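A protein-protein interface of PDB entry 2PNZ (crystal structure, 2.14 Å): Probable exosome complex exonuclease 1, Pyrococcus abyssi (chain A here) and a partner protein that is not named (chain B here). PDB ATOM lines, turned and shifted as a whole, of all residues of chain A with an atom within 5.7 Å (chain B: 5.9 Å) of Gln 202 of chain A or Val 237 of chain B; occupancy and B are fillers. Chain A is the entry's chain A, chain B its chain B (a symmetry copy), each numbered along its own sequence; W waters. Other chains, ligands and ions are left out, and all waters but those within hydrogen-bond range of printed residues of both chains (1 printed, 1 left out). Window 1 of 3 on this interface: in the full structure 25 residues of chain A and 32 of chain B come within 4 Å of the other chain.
The side-chain carboxylate of Glu 100 of chain A lies within salt-bridge range of the guanidinium group of Arg 115 of chain B.
The backbone NH (N) of Met 203 of chain A lies within hydrogen-bond range of the backbone carbonyl oxygen (O) of Val 237 of chain B (3.1 Å).
OE2 of Glu 100 of chain A sits at hydrogen-bond distance from NE2 of Gln 238 of chain B, 3.0 Å away.
The side-chain amide nitrogen of Gln 202 of chain A sits at hydrogen-bond distance from the side-chain amide oxygen of Gln 238 of chain B, 2.8 Å away.
The backbone carbonyl oxygen (O) of Leu 201 of chain A lies within hydrogen-bond range of the backbone NH (N) of Lys 239 of chain B (2.8 Å).
NH1 of Arg 137 of chain A lies within hydrogen-bond range of OE1 of Gln 202 of chain A (2.8 Å).
The backbone NH (N) of Asp 186 of chain A is in hydrogen-bond range of the backbone carbonyl oxygen (O) of Asp 204 of chain A (2.8 Å).
The backbone NH (N) of Thr 227 of chain B sits at hydrogen-bond distance from the backbone carbonyl oxygen (O) of Ala 236 of chain B, at 2.9 Å.
The side-chain carboxylate (OE2) of Glu 100 of chain A sits at hydrogen-bond distance from the side-chain amide nitrogen (NE2) of Gln 202 of chain A.
N of Thr 225 of chain B lies within hydrogen-bond range of O of Gln 238 of chain B.
N of Ser 235 of chain B is in hydrogen-bond range of O of Thr 227 of chain B, at 2.9 Å.
Gln 238 of chain B touches Val 104 of chain A (NE2 to CG2, 3.5 Å).
CG2 of Val 104 of chain A touches O of Lys 239 of chain B, at 3.8 Å.
O of Leu 201 of chain A touches CA of Gln 238 of chain B, at 3.6 Å.
CA of Gln 202 of chain A touches O of Val 237 of chain B, 3.3 Å away.
Met 203 of chain A touches Ile 234 of chain B (CE to O, 2.9 Å).
Met 203 of chain A touches Ala 236 of chain B (CE to N, 3.4 Å).
Arg 115 of chain B touches Asp 204 of chain A (CD to OD1, 3.3 Å).
Phe 212 of chain A touches Ile 234 of chain B.
CZ of Phe 212 of chain A touches CG2 of Val 237 of chain B (3.7 Å).
CG2 of Val 254 of chain B touches CE1 of Phe 212 of chain A, 3.7 Å away.
Of chain B, only Val 237 and Gln 238 come within 4 Å of Gln 202 of chain A.
Of the printed residues of chain A, Arg 115 of chain B touches Glu 100 and Asp 204.
Printed residues of chain A within 4 Å of Val 237 of chain B: Gln 202, Met 203 and Phe 212.
Of the printed residues of chain A, Val 254 of chain B touches Phe 212.
The nearest residue of chain B that does not touch Gln 202 of chain A is Arg 115 of chain B (4.1 Å).
The nearest printed residue of chain B that does not touch Asp 204 of chain A is Ser 235 of chain B (5.3 Å).
Printed residues of chain A that touch a printed residue of chain B: Glu 100, Val 104, Leu 201, Gln 202, Met 203, Asp 204 and Phe 212.
Hydrophobic or aromatic side chains of chain A within 4 Å of the printed part of chain B: Val 104, Met 203 and Phe 212.
Of the 13 printed residues of chain B, 8 touch a printed residue of chain A.
Among the printed residues, 16 pairs touch across the chains.
Among the printed residues, Asp or Glu carboxylates within 4 Å of a Lys or Arg side-chain nitrogen of the other chain: Glu 100 of chain A with Arg 115 of chain B.
Water W1 lies within hydrogen-bond range of the backbone carbonyl oxygen (O) of Lys 239 of chain B (2.7 Å) and the backbone NH (N) of Leu 201 of chain A (2.9 Å).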
ATOM      1  N   GLU A 100     -10.589 -20.143 -17.226  1.00  0.00           N
ATOM      2  CA  GLU A 100     -10.069 -19.847 -15.889  1.00  0.00           C
ATOM      3  C   GLU A 100     -10.805 -18.638 -15.285  1.00  0.00           C
ATOM      4  O   GLU A 100     -11.054 -18.583 -14.081  1.00  0.00           O
ATOM      5  CB  GLU A 100      -8.531 -19.665 -15.936  1.00  0.00           C
ATOM      6  CG  GLU A 100      -7.919 -19.308 -14.582  1.00  0.00           C
ATOM      7  CD  GLU A 100      -6.714 -18.363 -14.652  1.00  0.00           C
ATOM      8  OE1 GLU A 100      -6.208 -18.011 -15.730  1.00  0.00           O
ATOM      9  OE2 GLU A 100      -6.302 -17.877 -13.587  1.00  0.00           O
ATOM     10  N   VAL A 104     -12.747 -18.707 -11.704  1.00  0.00           N
ATOM     11  CA  VAL A 104     -12.359 -17.751 -10.646  1.00  0.00           C
ATOM     12  C   VAL A 104     -13.496 -16.743 -10.311  1.00  0.00           C
ATOM     13  O   VAL A 104     -13.639 -16.321  -9.136  1.00  0.00           O
ATOM     14  CB  VAL A 104     -10.970 -17.180 -11.123  1.00  0.00           C
ATOM     15  CG1 VAL A 104     -11.044 -15.832 -11.768  1.00  0.00           C
ATOM     16  CG2 VAL A 104      -9.868 -17.397 -10.177  1.00  0.00           C
ATOM     17  N   ARG A 137     -12.740  -8.979 -15.769  1.00  0.00           N
ATOM     18  CA  ARG A 137     -13.185 -10.007 -14.860  1.00  0.00           C
ATOM     19  C   ARG A 137     -13.753  -9.403 -13.556  1.00  0.00           C
ATOM     20  O   ARG A 137     -14.814  -9.797 -13.085  1.00  0.00           O
ATOM     21  CB  ARG A 137     -12.085 -11.052 -14.626  1.00  0.00           C
ATOM     22  CG  ARG A 137     -11.119 -10.781 -13.503  1.00  0.00           C
ATOM     23  CD  ARG A 137      -9.982 -11.808 -13.534  1.00  0.00           C
ATOM     24  NE  ARG A 137      -9.321 -11.800 -14.821  1.00  0.00           N
ATOM     25  CZ  ARG A 137      -8.162 -12.390 -15.080  1.00  0.00           C
ATOM     26  NH1 ARG A 137      -7.483 -12.992 -14.121  1.00  0.00           N
ATOM     27  NH2 ARG A 137      -7.671 -12.366 -16.308  1.00  0.00           N
ATOM     28  N   ASP A 186      -0.714  -7.054 -12.450  1.00  0.00           N
ATOM     29  CA  ASP A 186      -2.104  -6.799 -12.417  1.00  0.00           C
ATOM     30  C   ASP A 186      -2.621  -7.674 -11.243  1.00  0.00           C
ATOM     31  O   ASP A 186      -2.262  -8.878 -11.093  1.00  0.00           O
ATOM     32  CB  ASP A 186      -2.706  -7.248 -13.740  1.00  0.00           C
ATOM     33  CG  ASP A 186      -4.168  -6.870 -13.881  1.00  0.00           C
ATOM     34  OD1 ASP A 186      -4.846  -7.552 -14.667  1.00  0.00           O
ATOM     35  OD2 ASP A 186      -4.645  -5.914 -13.216  1.00  0.00           O
ATOM     36  N   VAL A 187      -3.441  -7.042 -10.404  1.00  0.00           N
ATOM     37  CA  VAL A 187      -3.943  -7.665  -9.189  1.00  0.00           C
ATOM     38  C   VAL A 187      -5.439  -7.397  -9.053  1.00  0.00           C
ATOM     39  O   VAL A 187      -5.843  -6.385  -8.395  1.00  0.00           O
ATOM     40  CB  VAL A 187      -3.144  -7.164  -7.944  1.00  0.00           C
ATOM     41  CG1 VAL A 187      -3.462  -7.944  -6.726  1.00  0.00           C
ATOM     42  CG2 VAL A 187      -1.667  -7.252  -8.218  1.00  0.00           C
ATOM     43  N   PRO A 188      -6.266  -8.235  -9.696  1.00  0.00           N
ATOM     44  CA  PRO A 188      -7.687  -8.131  -9.376  1.00  0.00           C
ATOM     45  C   PRO A 188      -8.011  -8.750  -8.037  1.00  0.00           C
ATOM     46  O   PRO A 188      -7.310  -9.653  -7.567  1.00  0.00           O
ATOM     47  CB  PRO A 188      -8.367  -8.949 -10.467  1.00  0.00           C
ATOM     48  CG  PRO A 188      -7.374  -9.915 -10.870  1.00  0.00           C
ATOM     49  CD  PRO A 188      -6.047  -9.292 -10.730  1.00  0.00           C
ATOM     50  N   VAL A 189      -9.051  -8.208  -7.412  1.00  0.00           N
ATOM     51  CA  VAL A 189      -9.425  -8.602  -6.069  1.00  0.00           C
ATOM     52  C   VAL A 189     -10.931  -8.490  -6.114  1.00  0.00           C
ATOM     53  O   VAL A 189     -11.486  -7.568  -6.717  1.00  0.00           O
ATOM     54  CB  VAL A 189      -8.852  -7.632  -5.044  1.00  0.00           C
ATOM     55  CG1 VAL A 189      -9.271  -7.982  -3.655  1.00  0.00           C
ATOM     56  CG2 VAL A 189      -7.343  -7.617  -5.121  1.00  0.00           C
ATOM     57  N   LEU A 200     -11.895 -13.122  -4.583  1.00  0.00           N
ATOM     58  CA  LEU A 200     -11.046 -13.373  -5.734  1.00  0.00           C
ATOM     59  C   LEU A 200      -9.765 -12.717  -5.425  1.00  0.00           C
ATOM     60  O   LEU A 200      -9.740 -11.610  -4.926  1.00  0.00           O
ATOM     61  CB  LEU A 200     -11.634 -12.825  -7.030  1.00  0.00           C
ATOM     62  CG  LEU A 200     -10.787 -12.792  -8.349  1.00  0.00           C
ATOM     63  CD1 LEU A 200     -11.623 -13.108  -9.559  1.00  0.00           C
ATOM     64  CD2 LEU A 200      -9.940 -11.560  -8.666  1.00  0.00           C
ATOM     65  N   LEU A 201      -8.664 -13.375  -5.749  1.00  0.00           N
ATOM     66  CA  LEU A 201      -7.393 -12.682  -5.623  1.00  0.00           C
ATOM     67  C   LEU A 201      -6.465 -13.376  -6.582  1.00  0.00           C
ATOM     68  O   LEU A 201      -6.240 -14.543  -6.466  1.00  0.00           O
ATOM     69  CB  LEU A 201      -6.823 -12.687  -4.195  1.00  0.00           C
ATOM     70  CG  LEU A 201      -5.952 -11.531  -3.638  1.00  0.00           C
ATOM     71  CD1 LEU A 201      -4.901 -12.011  -2.631  1.00  0.00           C
ATOM     72  CD2 LEU A 201      -5.243 -10.779  -4.722  1.00  0.00           C
ATOM     73  N   GLN A 202      -6.009 -12.601  -7.552  1.00  0.00           N
ATOM     74  CA  GLN A 202      -5.096 -13.034  -8.576  1.00  0.00           C
ATOM     75  C   GLN A 202      -4.029 -11.959  -8.679  1.00  0.00           C
ATOM     76  O   GLN A 202      -4.233 -10.812  -8.283  1.00  0.00           O
ATOM     77  CB  GLN A 202      -5.841 -13.230  -9.915  1.00  0.00           C
ATOM     78  CG  GLN A 202      -6.894 -14.290  -9.805  1.00  0.00           C
ATOM     79  CD  GLN A 202      -7.496 -14.599 -11.137  1.00  0.00           C
ATOM     80  OE1 GLN A 202      -8.335 -13.842 -11.640  1.00  0.00           O
ATOM     81  NE2 GLN A 202      -7.075 -15.700 -11.723  1.00  0.00           N
ATOM     82  N   MET A 203      -2.876 -12.406  -9.119  1.00  0.00           N
ATOM     83  CA  MET A 203      -1.726 -11.603  -9.344  1.00  0.00           C
ATOM     84  C   MET A 203      -1.050 -12.237 -10.525  1.00  0.00           C
ATOM     85  O   MET A 203      -0.663 -13.401 -10.491  1.00  0.00           O
ATOM     86  CB  MET A 203      -0.792 -11.570  -8.091  1.00  0.00           C
ATOM     87  CG  MET A 203       0.233 -10.507  -8.155  1.00  0.00           C
ATOM     88  SD  MET A 203       1.630 -10.829  -9.272  1.00  0.00           S
ATOM     89  CE  MET A 203       2.680 -11.845  -8.312  1.00  0.00           C
ATOM     90  N   ASP A 204      -0.991 -11.456 -11.594  1.00  0.00           N
ATOM     91  CA  ASP A 204      -0.302 -11.769 -12.835  1.00  0.00           C
ATOM     92  C   ASP A 204       0.825 -10.760 -12.846  1.00  0.00           C
ATOM     93  O   ASP A 204       0.573  -9.542 -12.741  1.00  0.00           O
ATOM     94  CB  ASP A 204      -1.221 -11.397 -13.970  1.00  0.00           C
ATOM     95  CG  ASP A 204      -0.819 -12.012 -15.256  1.00  0.00           C
ATOM     96  OD1 ASP A 204       0.245 -12.671 -15.311  1.00  0.00           O
ATOM     97  OD2 ASP A 204      -1.566 -11.853 -16.253  1.00  0.00           O
ATOM     98  N   PHE A 212       2.859  -6.251  -3.444  1.00  0.00           N
ATOM     99  CA  PHE A 212       1.661  -7.056  -3.671  1.00  0.00           C
ATOM    100  C   PHE A 212       0.540  -6.708  -2.683  1.00  0.00           C
ATOM    101  O   PHE A 212      -0.580  -6.507  -3.105  1.00  0.00           O
ATOM    102  CB  PHE A 212       1.960  -8.576  -3.729  1.00  0.00           C
ATOM    103  CG  PHE A 212       0.722  -9.417  -3.629  1.00  0.00           C
ATOM    104  CD1 PHE A 212       0.460 -10.133  -2.473  1.00  0.00           C
ATOM    105  CD2 PHE A 212      -0.215  -9.456  -4.693  1.00  0.00           C
ATOM    106  CE1 PHE A 212      -0.677 -10.859  -2.356  1.00  0.00           C
ATOM    107  CE2 PHE A 212      -1.354 -10.202  -4.599  1.00  0.00           C
ATOM    108  CZ  PHE A 212      -1.607 -10.913  -3.437  1.00  0.00           C
ATOM    109  N   VAL B 112      -1.756 -21.142 -14.072  1.00  0.00           N
ATOM    110  CA  VAL B 112      -1.148 -20.535 -12.888  1.00  0.00           C
ATOM    111  C   VAL B 112       0.292 -20.951 -12.762  1.00  0.00           C
ATOM    112  O   VAL B 112       1.087 -20.193 -12.209  1.00  0.00           O
ATOM    113  CB  VAL B 112      -1.851 -20.877 -11.540  1.00  0.00           C
ATOM    114  CG1 VAL B 112      -1.008 -20.366 -10.346  1.00  0.00           C
ATOM    115  CG2 VAL B 112      -3.168 -20.307 -11.468  1.00  0.00           C
ATOM    116  N   ARG B 115       2.004 -18.989 -15.477  1.00  0.00           N
ATOM    117  CA  ARG B 115       2.177 -17.528 -15.115  1.00  0.00           C
ATOM    118  C   ARG B 115       3.382 -17.365 -14.162  1.00  0.00           C
ATOM    119  O   ARG B 115       4.165 -16.396 -14.263  1.00  0.00           O
ATOM    120  CB  ARG B 115       0.939 -16.899 -14.460  1.00  0.00           C
ATOM    121  CG  ARG B 115      -0.134 -16.638 -15.467  1.00  0.00           C
ATOM    122  CD  ARG B 115      -1.141 -15.703 -14.984  1.00  0.00           C
ATOM    123  NE  ARG B 115      -1.823 -16.229 -13.822  1.00  0.00           N
ATOM    124  CZ  ARG B 115      -2.951 -16.919 -13.918  1.00  0.00           C
ATOM    125  NH1 ARG B 115      -3.540 -17.373 -12.839  1.00  0.00           N
ATOM    126  NH2 ARG B 115      -3.454 -17.183 -15.120  1.00  0.00           N
ATOM    127  N   ILE B 224      -5.609 -20.779  -1.533  1.00  0.00           N
ATOM    128  CA  ILE B 224      -4.873 -19.714  -2.178  1.00  0.00           C
ATOM    129  C   ILE B 224      -3.464 -20.195  -2.423  1.00  0.00           C
ATOM    130  O   ILE B 224      -2.937 -20.922  -1.636  1.00  0.00           O
ATOM    131  CB  ILE B 224      -4.898 -18.401  -1.318  1.00  0.00           C
ATOM    132  CG1 ILE B 224      -4.298 -17.222  -2.081  1.00  0.00           C
ATOM    133  CG2 ILE B 224      -4.243 -18.622   0.083  1.00  0.00           C
ATOM    134  CD1 ILE B 224      -4.327 -15.878  -1.284  1.00  0.00           C
ATOM    135  N   THR B 225      -2.896 -19.840  -3.571  1.00  0.00           N
ATOM    136  CA  THR B 225      -1.567 -20.343  -3.966  1.00  0.00           C
ATOM    137  C   THR B 225      -0.719 -19.124  -4.175  1.00  0.00           C
ATOM    138  O   THR B 225      -1.184 -18.190  -4.781  1.00  0.00           O
ATOM    139  CB  THR B 225      -1.633 -21.030  -5.358  1.00  0.00           C
ATOM    140  OG1 THR B 225      -2.264 -22.309  -5.245  1.00  0.00           O
ATOM    141  CG2 THR B 225      -0.241 -21.169  -5.932  1.00  0.00           C
ATOM    142  N   ILE B 226       0.516 -19.162  -3.668  1.00  0.00           N
ATOM    143  CA  ILE B 226       1.431 -18.060  -3.817  1.00  0.00           C
ATOM    144  C   ILE B 226       2.767 -18.540  -4.379  1.00  0.00           C
ATOM    145  O   ILE B 226       3.452 -19.330  -3.786  1.00  0.00           O
ATOM    146  CB  ILE B 226       1.733 -17.314  -2.488  1.00  0.00           C
ATOM    147  CG1 ILE B 226       0.460 -17.151  -1.620  1.00  0.00           C
ATOM    148  CG2 ILE B 226       2.461 -16.004  -2.818  1.00  0.00           C
ATOM    149  CD1 ILE B 226      -0.428 -15.958  -2.028  1.00  0.00           C
ATOM    150  N   THR B 227       3.120 -18.048  -5.543  1.00  0.00           N
ATOM    151  CA  THR B 227       4.302 -18.521  -6.137  1.00  0.00           C
ATOM    152  C   THR B 227       5.331 -17.463  -6.025  1.00  0.00           C
ATOM    153  O   THR B 227       5.100 -16.344  -6.437  1.00  0.00           O
ATOM    154  CB  THR B 227       4.017 -18.842  -7.612  1.00  0.00           C
ATOM    155  OG1 THR B 227       2.930 -19.720  -7.597  1.00  0.00           O
ATOM    156  CG2 THR B 227       5.225 -19.529  -8.264  1.00  0.00           C
ATOM    157  N   ILE B 234       6.988 -12.247  -5.844  1.00  0.00           N
ATOM    158  CA  ILE B 234       5.830 -13.044  -6.149  1.00  0.00           C
ATOM    159  C   ILE B 234       5.617 -12.944  -7.590  1.00  0.00           C
ATOM    160  O   ILE B 234       5.590 -11.841  -8.141  1.00  0.00           O
ATOM    161  CB  ILE B 234       4.555 -12.561  -5.419  1.00  0.00           C
ATOM    162  CG1 ILE B 234       4.848 -12.307  -3.947  1.00  0.00           C
ATOM    163  CG2 ILE B 234       3.482 -13.650  -5.509  1.00  0.00           C
ATOM    164  CD1 ILE B 234       3.918 -11.318  -3.325  1.00  0.00           C
ATOM    165  N   SER B 235       5.487 -14.078  -8.238  1.00  0.00           N
ATOM    166  CA  SER B 235       5.143 -14.109  -9.681  1.00  0.00           C
ATOM    167  C   SER B 235       3.856 -14.737 -10.019  1.00  0.00           C
ATOM    168  O   SER B 235       3.590 -14.938 -11.192  1.00  0.00           O
ATOM    169  CB  SER B 235       6.166 -14.863 -10.457  1.00  0.00           C
ATOM    170  OG  SER B 235       6.301 -16.142  -9.947  1.00  0.00           O
ATOM    171  N   ALA B 236       3.075 -15.134  -9.022  1.00  0.00           N
ATOM    172  CA  ALA B 236       1.693 -15.586  -9.274  1.00  0.00           C
ATOM    173  C   ALA B 236       1.044 -15.607  -7.950  1.00  0.00           C
ATOM    174  O   ALA B 236       1.657 -16.034  -6.962  1.00  0.00           O
ATOM    175  CB  ALA B 236       1.671 -17.006  -9.769  1.00  0.00           C
ATOM    176  N   VAL B 237      -0.222 -15.217  -7.954  1.00  0.00           N
ATOM    177  CA  VAL B 237      -1.137 -15.510  -6.861  1.00  0.00           C
ATOM    178  C   VAL B 237      -2.418 -15.944  -7.520  1.00  0.00           C
ATOM    179  O   VAL B 237      -2.832 -15.430  -8.580  1.00  0.00           O
ATOM    180  CB  VAL B 237      -1.401 -14.281  -5.896  1.00  0.00           C
ATOM    181  CG1 VAL B 237      -2.298 -14.688  -4.693  1.00  0.00           C
ATOM    182  CG2 VAL B 237      -0.116 -13.745  -5.373  1.00  0.00           C
ATOM    183  N   GLN B 238      -3.023 -16.916  -6.876  1.00  0.00           N
ATOM    184  CA  GLN B 238      -4.276 -17.442  -7.267  1.00  0.00           C
ATOM    185  C   GLN B 238      -5.029 -17.953  -6.025  1.00  0.00           C
ATOM    186  O   GLN B 238      -4.675 -18.978  -5.435  1.00  0.00           O
ATOM    187  CB  GLN B 238      -4.065 -18.661  -8.192  1.00  0.00           C
ATOM    188  CG  GLN B 238      -5.393 -19.062  -8.790  1.00  0.00           C
ATOM    189  CD  GLN B 238      -5.792 -18.358 -10.079  1.00  0.00           C
ATOM    190  OE1 GLN B 238      -5.263 -17.324 -10.429  1.00  0.00           O
ATOM    191  NE2 GLN B 238      -6.763 -18.945 -10.801  1.00  0.00           N
ATOM    192  N   LYS B 239      -6.091 -17.266  -5.670  1.00  0.00           N
ATOM    193  CA  LYS B 239      -7.097 -17.776  -4.745  1.00  0.00           C
ATOM    194  C   LYS B 239      -7.923 -18.578  -5.728  1.00  0.00           C
ATOM    195  O   LYS B 239      -8.305 -18.062  -6.800  1.00  0.00           O
ATOM    196  CB  LYS B 239      -7.911 -16.607  -4.262  1.00  0.00           C
ATOM    197  CG  LYS B 239      -9.011 -16.853  -3.250  1.00  0.00           C
ATOM    198  CD  LYS B 239     -10.209 -17.608  -3.804  1.00  0.00           C
ATOM    199  CE  LYS B 239     -11.355 -17.716  -2.835  1.00  0.00           C
ATOM    200  NZ  LYS B 239     -12.679 -17.428  -3.588  1.00  0.00           N
ATOM    201  N   VAL B 254       1.524 -15.160   2.152  1.00  0.00           N
ATOM    202  CA  VAL B 254       2.615 -14.695   1.299  1.00  0.00           C
ATOM    203  C   VAL B 254       3.926 -14.939   2.052  1.00  0.00           C
ATOM    204  O   VAL B 254       4.904 -15.463   1.499  1.00  0.00           O
ATOM    205  CB  VAL B 254       2.425 -13.174   0.956  1.00  0.00           C
ATOM    206  CG1 VAL B 254       3.691 -12.580   0.388  1.00  0.00           C
ATOM    207  CG2 VAL B 254       1.242 -12.984  -0.027  1.00  0.00           C
HETATM  208  O   HOH W   1      -9.383 -15.649  -7.331  1.00  0.00           O
